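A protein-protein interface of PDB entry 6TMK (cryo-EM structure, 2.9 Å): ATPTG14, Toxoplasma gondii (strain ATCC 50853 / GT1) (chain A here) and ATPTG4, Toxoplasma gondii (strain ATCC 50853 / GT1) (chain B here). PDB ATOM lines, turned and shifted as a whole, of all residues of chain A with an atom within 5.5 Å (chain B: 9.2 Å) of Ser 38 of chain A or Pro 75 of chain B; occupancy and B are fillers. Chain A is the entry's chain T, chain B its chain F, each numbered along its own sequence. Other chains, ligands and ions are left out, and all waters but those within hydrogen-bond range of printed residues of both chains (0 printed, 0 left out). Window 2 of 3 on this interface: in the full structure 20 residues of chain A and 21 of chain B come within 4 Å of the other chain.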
ATOM      1  N   PRO A  34     -23.699 -31.377 -21.458  1.00  0.00           N
ATOM      2  CA  PRO A  34     -24.584 -31.081 -20.330  1.00  0.00           C
ATOM      3  C   PRO A  34     -25.942 -31.749 -20.475  1.00  0.00           C
ATOM      4  O   PRO A  34     -26.362 -32.159 -21.559  1.00  0.00           O
ATOM      5  CB  PRO A  34     -24.704 -29.557 -20.365  1.00  0.00           C
ATOM      6  CG  PRO A  34     -24.528 -29.212 -21.785  1.00  0.00           C
ATOM      7  CD  PRO A  34     -23.568 -30.220 -22.359  1.00  0.00           C
ATOM      8  N   THR A  35     -26.630 -31.849 -19.341  1.00  0.00           N
ATOM      9  CA  THR A  35     -27.892 -32.561 -19.219  1.00  0.00           C
ATOM     10  C   THR A  35     -28.900 -31.671 -18.505  1.00  0.00           C
ATOM     11  O   THR A  35     -28.600 -30.541 -18.111  1.00  0.00           O
ATOM     12  CB  THR A  35     -27.710 -33.880 -18.461  1.00  0.00           C
ATOM     13  OG1 THR A  35     -27.146 -33.619 -17.172  1.00  0.00           O
ATOM     14  CG2 THR A  35     -26.795 -34.803 -19.224  1.00  0.00           C
ATOM     15  N   ALA A  36     -30.113 -32.193 -18.341  1.00  0.00           N
ATOM     16  CA  ALA A  36     -31.151 -31.500 -17.595  1.00  0.00           C
ATOM     17  C   ALA A  36     -30.994 -31.631 -16.087  1.00  0.00           C
ATOM     18  O   ALA A  36     -31.769 -31.019 -15.346  1.00  0.00           O
ATOM     19  CB  ALA A  36     -32.523 -32.031 -18.008  1.00  0.00           C
ATOM     20  N   GLY A  37     -30.025 -32.410 -15.614  1.00  0.00           N
ATOM     21  CA  GLY A  37     -29.838 -32.587 -14.188  1.00  0.00           C
ATOM     22  C   GLY A  37     -29.084 -31.474 -13.503  1.00  0.00           C
ATOM     23  O   GLY A  37     -29.019 -31.452 -12.272  1.00  0.00           O
ATOM     24  N   SER A  38     -28.510 -30.555 -14.274  1.00  0.00           N
ATOM     25  CA  SER A  38     -27.748 -29.435 -13.742  1.00  0.00           C
ATOM     26  C   SER A  38     -28.479 -28.110 -13.889  1.00  0.00           C
ATOM     27  O   SER A  38     -27.907 -27.061 -13.578  1.00  0.00           O
ATOM     28  CB  SER A  38     -26.388 -29.355 -14.435  1.00  0.00           C
ATOM     29  OG  SER A  38     -26.540 -29.226 -15.835  1.00  0.00           O
ATOM     30  N   CYS A  39     -29.724 -28.129 -14.350  1.00  0.00           N
ATOM     31  CA  CYS A  39     -30.432 -26.911 -14.703  1.00  0.00           C
ATOM     32  C   CYS A  39     -31.923 -27.133 -14.513  1.00  0.00           C
ATOM     33  O   CYS A  39     -32.376 -28.237 -14.200  1.00  0.00           O
ATOM     34  CB  CYS A  39     -30.143 -26.503 -16.145  1.00  0.00           C
ATOM     35  SG  CYS A  39     -30.702 -27.716 -17.351  1.00  0.00           S
ATOM     36  N   ALA A  40     -32.689 -26.067 -14.710  1.00  0.00           N
ATOM     37  CA  ALA A  40     -34.132 -26.169 -14.625  1.00  0.00           C
ATOM     38  C   ALA A  40     -34.679 -26.886 -15.848  1.00  0.00           C
ATOM     39  O   ALA A  40     -34.124 -26.807 -16.945  1.00  0.00           O
ATOM     40  CB  ALA A  40     -34.757 -24.783 -14.517  1.00  0.00           C
ATOM     41  N   GLN A  66     -30.652 -30.035  -7.764  1.00  0.00           N
ATOM     42  CA  GLN A  66     -29.731 -30.139  -8.886  1.00  0.00           C
ATOM     43  C   GLN A  66     -28.296 -29.894  -8.453  1.00  0.00           C
ATOM     44  O   GLN A  66     -27.374 -30.525  -8.982  1.00  0.00           O
ATOM     45  CB  GLN A  66     -30.119 -29.146  -9.978  1.00  0.00           C
ATOM     46  CG  GLN A  66     -31.385 -29.497 -10.719  1.00  0.00           C
ATOM     47  CD  GLN A  66     -32.628 -29.002 -10.030  1.00  0.00           C
ATOM     48  OE1 GLN A  66     -32.561 -28.285  -9.036  1.00  0.00           O
ATOM     49  NE2 GLN A  66     -33.780 -29.387 -10.557  1.00  0.00           N
ATOM     50  N   GLU A  70     -26.012 -32.963  -9.861  1.00  0.00           N
ATOM     51  CA  GLU A  70     -25.122 -32.728 -10.989  1.00  0.00           C
ATOM     52  C   GLU A  70     -23.883 -33.610 -10.939  1.00  0.00           C
ATOM     53  O   GLU A  70     -23.242 -33.819 -11.974  1.00  0.00           O
ATOM     54  CB  GLU A  70     -24.708 -31.261 -11.022  1.00  0.00           C
ATOM     55  CG  GLU A  70     -23.735 -30.884  -9.930  1.00  0.00           C
ATOM     56  CD  GLU A  70     -23.753 -29.402  -9.616  1.00  0.00           C
ATOM     57  OE1 GLU A  70     -24.182 -28.613 -10.484  1.00  0.00           O
ATOM     58  OE2 GLU A  70     -23.334 -29.025  -8.501  1.00  0.00           O
ATOM     59  N   ASP A  73     -25.329 -37.541 -11.744  1.00  0.00           N
ATOM     60  CA  ASP A  73     -26.201 -37.642 -12.912  1.00  0.00           C
ATOM     61  C   ASP A  73     -26.084 -38.977 -13.645  1.00  0.00           C
ATOM     62  O   ASP A  73     -27.049 -39.417 -14.281  1.00  0.00           O
ATOM     63  CB  ASP A  73     -25.875 -36.496 -13.870  1.00  0.00           C
ATOM     64  CG  ASP A  73     -27.084 -36.006 -14.631  1.00  0.00           C
ATOM     65  OD1 ASP A  73     -28.071 -36.762 -14.745  1.00  0.00           O
ATOM     66  OD2 ASP A  73     -27.046 -34.860 -15.124  1.00  0.00           O
ATOM     67  N   PHE B  72     -29.878 -18.610  -3.363  1.00  0.00           N
ATOM     68  CA  PHE B  72     -30.230 -19.827  -4.074  1.00  0.00           C
ATOM     69  C   PHE B  72     -30.575 -19.502  -5.515  1.00  0.00           C
ATOM     70  O   PHE B  72     -31.309 -18.548  -5.789  1.00  0.00           O
ATOM     71  CB  PHE B  72     -31.409 -20.534  -3.416  1.00  0.00           C
ATOM     72  CG  PHE B  72     -31.899 -21.719  -4.179  1.00  0.00           C
ATOM     73  CD1 PHE B  72     -31.270 -22.941  -4.066  1.00  0.00           C
ATOM     74  CD2 PHE B  72     -32.996 -21.611  -5.008  1.00  0.00           C
ATOM     75  CE1 PHE B  72     -31.726 -24.029  -4.768  1.00  0.00           C
ATOM     76  CE2 PHE B  72     -33.453 -22.695  -5.709  1.00  0.00           C
ATOM     77  CZ  PHE B  72     -32.820 -23.903  -5.591  1.00  0.00           C
ATOM     78  N   ALA B  73     -30.045 -20.304  -6.434  1.00  0.00           N
ATOM     79  CA  ALA B  73     -30.297 -20.098  -7.847  1.00  0.00           C
ATOM     80  C   ALA B  73     -30.209 -21.428  -8.572  1.00  0.00           C
ATOM     81  O   ALA B  73     -29.543 -22.362  -8.117  1.00  0.00           O
ATOM     82  CB  ALA B  73     -29.302 -19.109  -8.453  1.00  0.00           C
ATOM     83  N   ILE B  74     -30.894 -21.499  -9.704  1.00  0.00           N
ATOM     84  CA  ILE B  74     -30.803 -22.631 -10.617  1.00  0.00           C
ATOM     85  C   ILE B  74     -30.566 -22.031 -11.996  1.00  0.00           C
ATOM     86  O   ILE B  74     -31.238 -21.056 -12.357  1.00  0.00           O
ATOM     87  CB  ILE B  74     -32.064 -23.504 -10.567  1.00  0.00           C
ATOM     88  CG1 ILE B  74     -32.189 -24.164  -9.198  1.00  0.00           C
ATOM     89  CG2 ILE B  74     -32.008 -24.567 -11.624  1.00  0.00           C
ATOM     90  CD1 ILE B  74     -33.574 -24.623  -8.869  1.00  0.00           C
ATOM     91  N   PRO B  75     -29.641 -22.554 -12.797  1.00  0.00           N
ATOM     92  CA  PRO B  75     -29.455 -22.002 -14.131  1.00  0.00           C
ATOM     93  C   PRO B  75     -30.719 -22.142 -14.952  1.00  0.00           C
ATOM     94  O   PRO B  75     -31.535 -23.054 -14.722  1.00  0.00           O
ATOM     95  CB  PRO B  75     -28.306 -22.841 -14.709  1.00  0.00           C
ATOM     96  CG  PRO B  75     -28.021 -23.907 -13.714  1.00  0.00           C
ATOM     97  CD  PRO B  75     -28.549 -23.460 -12.418  1.00  0.00           C
ATOM     98  N   PRO B  76     -30.921 -21.262 -15.934  1.00  0.00           N
ATOM     99  CA  PRO B  76     -32.258 -21.153 -16.540  1.00  0.00           C
ATOM    100  C   PRO B  76     -32.708 -22.410 -17.260  1.00  0.00           C
ATOM    101  O   PRO B  76     -33.803 -22.918 -16.993  1.00  0.00           O
ATOM    102  CB  PRO B  76     -32.102 -19.963 -17.495  1.00  0.00           C
ATOM    103  CG  PRO B  76     -30.646 -19.904 -17.787  1.00  0.00           C
ATOM    104  CD  PRO B  76     -29.967 -20.317 -16.532  1.00  0.00           C
ATOM    105  N   ALA B  77     -31.897 -22.918 -18.181  1.00  0.00           N
ATOM    106  CA  ALA B  77     -32.216 -24.150 -18.891  1.00  0.00           C
ATOM    107  C   ALA B  77     -31.074 -24.536 -19.819  1.00  0.00           C
ATOM    108  O   ALA B  77     -30.068 -23.826 -19.909  1.00  0.00           O
ATOM    109  CB  ALA B  77     -33.515 -24.010 -19.680  1.00  0.00           C
ATOM    110  N   ASN B  78     -31.224 -25.659 -20.514  1.00  0.00           N
ATOM    111  CA  ASN B  78     -30.243 -26.109 -21.485  1.00  0.00           C
ATOM    112  C   ASN B  78     -30.966 -26.563 -22.741  1.00  0.00           C
ATOM    113  O   ASN B  78     -32.169 -26.834 -22.729  1.00  0.00           O
ATOM    114  CB  ASN B  78     -29.381 -27.251 -20.936  1.00  0.00           C
ATOM    115  CG  ASN B  78     -28.316 -26.770 -19.982  1.00  0.00           C
ATOM    116  OD1 ASN B  78     -28.013 -25.579 -19.919  1.00  0.00           O
ATOM    117  ND2 ASN B  78     -27.742 -27.695 -19.225  1.00  0.00           N
ATOM    118  N   ALA B  79     -30.210 -26.634 -23.836  1.00  0.00           N
ATOM    119  CA  ALA B  79     -30.761 -27.168 -25.073  1.00  0.00           C
ATOM    120  C   ALA B  79     -31.272 -28.587 -24.876  1.00  0.00           C
ATOM    121  O   ALA B  79     -32.281 -28.980 -25.471  1.00  0.00           O
ATOM    122  CB  ALA B  79     -29.703 -27.127 -26.169  1.00  0.00           C
ATOM    123  N   ALA B  80     -30.593 -29.368 -24.037  1.00  0.00           N
ATOM    124  CA  ALA B  80     -31.054 -30.721 -23.749  1.00  0.00           C
ATOM    125  C   ALA B  80     -32.409 -30.699 -23.059  1.00  0.00           C
ATOM    126  O   ALA B  80     -33.330 -31.426 -23.448  1.00  0.00           O
ATOM    127  CB  ALA B  80     -30.027 -31.445 -22.887  1.00  0.00           C
ATOM    128  N   ALA B  81     -32.547 -29.870 -22.026  1.00  0.00           N
ATOM    129  CA  ALA B  81     -33.809 -29.799 -21.300  1.00  0.00           C
ATOM    130  C   ALA B  81     -34.937 -29.314 -22.198  1.00  0.00           C
ATOM    131  O   ALA B  81     -36.058 -29.827 -22.132  1.00  0.00           O
ATOM    132  CB  ALA B  81     -33.662 -28.885 -20.088  1.00  0.00           C
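The backbone carbonyl oxygen (O) of Thr 35 of chain A lies within hydrogen-bond range of the side-chain sulfur (SG) of Cys 39 of chain A (3.6 Å). The backbone NH (N) of Gly 37 of chain A lies close to the side-chain hydroxyl (OG1) of Thr 35 of chain A. The backbone carbonyl oxygen (O) of Thr 35 of chain A sits at hydrogen-bond distance from the side-chain hydroxyl (OG) of Ser 38 of chain A (3.3 Å).
Along chain B the printed residues that touch a printed residue of chain A span positions 74 to 81. Among the printed residues, 15 pairs touch across the chains. Among the printed residues, no Asp or Glu carboxylate lies within 4 Å of a Lys or Arg side-chain nitrogen of the other chain.
The side-chain amide nitrogen (ND2) of Asn 78 of chain B is in hydrogen-bond range of the backbone carbonyl oxygen (O) of Thr 35 of chain A (3.2 Å). ND2 of Asn 78 of chain B sits at hydrogen-bond distance from SG of Cys 39 of chain A, at 3.5 Å. The backbone carbonyl oxygen (O) of Pro 75 of chain B is in hydrogen-bond range of the backbone NH (N) of Ala 40 of chain A, 3.2 Å away.
Of chain B, only Pro 75 (3.2 Å) and Asn 78 (3.9 Å) come within 4 Å of Ser 38 of chain A. Pro 75 of chain B touches just these residues of chain A: Ser 38, Cys 39 and Ala 40. Cys 39 of chain A touches just these residues of chain B: Ile 74, Pro 75 and Asn 78. Ala 40 of chain A touches five residues of chain B. Printed residues of chain B within 4 Å of Thr 35 of chain A: Asn 78 (3.2 Å). Printed residues of chain B within 4 Å of Pro 34 of chain A: Asn 78 and Ala 80. Of the printed residues of chain A, Asn 78 of chain B touches Pro 34 (3.7 Å), Thr 35 (3.2 Å), Ser 38 (3.9 Å) and Cys 39 (3.5 Å). Of the printed residues of chain A, Ala 77 of chain B touches Ala 40 (3.8 Å). Printed residues of chain A within 4 Å of Ile 74 of chain B: Cys 39, Ala 40 and Gln 66. The nearest residue of chain B that does not touch Ser 38 of chain A is Ile 74 of chain B (5.2 Å).
Among the printed residues, pairs that only touch across the chains: Ser 38 of chain A with Pro 75 of chain B (3.2 Å), Ala 40 of chain A with Pro 76 of chain B (3.2 Å), Ala 40 of chain A with Ile 74 of chain B (3.5 Å), Pro 34 of chain A with Asn 78 of chain B (3.7 Å), Ala 40 of chain A with Ala 81 of chain B (3.8 Å), Gln 66 of chain A with Ile 74 of chain B (3.8 Å), Ala 40 of chain A with Ala 77 of chain B (3.8 Å), Cys 39 of chain A with Ile 74 of chain B (3.9 Å), Ser 38 of chain A with Asn 78 of chain B (3.9 Å), Ala 36 of chain A with Ala 81 of chain B (3.9 Å), Pro 34 of chain A with Ala 80 of chain B (3.96 Å) and Cys 39 of chain A with Pro 75 of chain B (3.98 Å).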
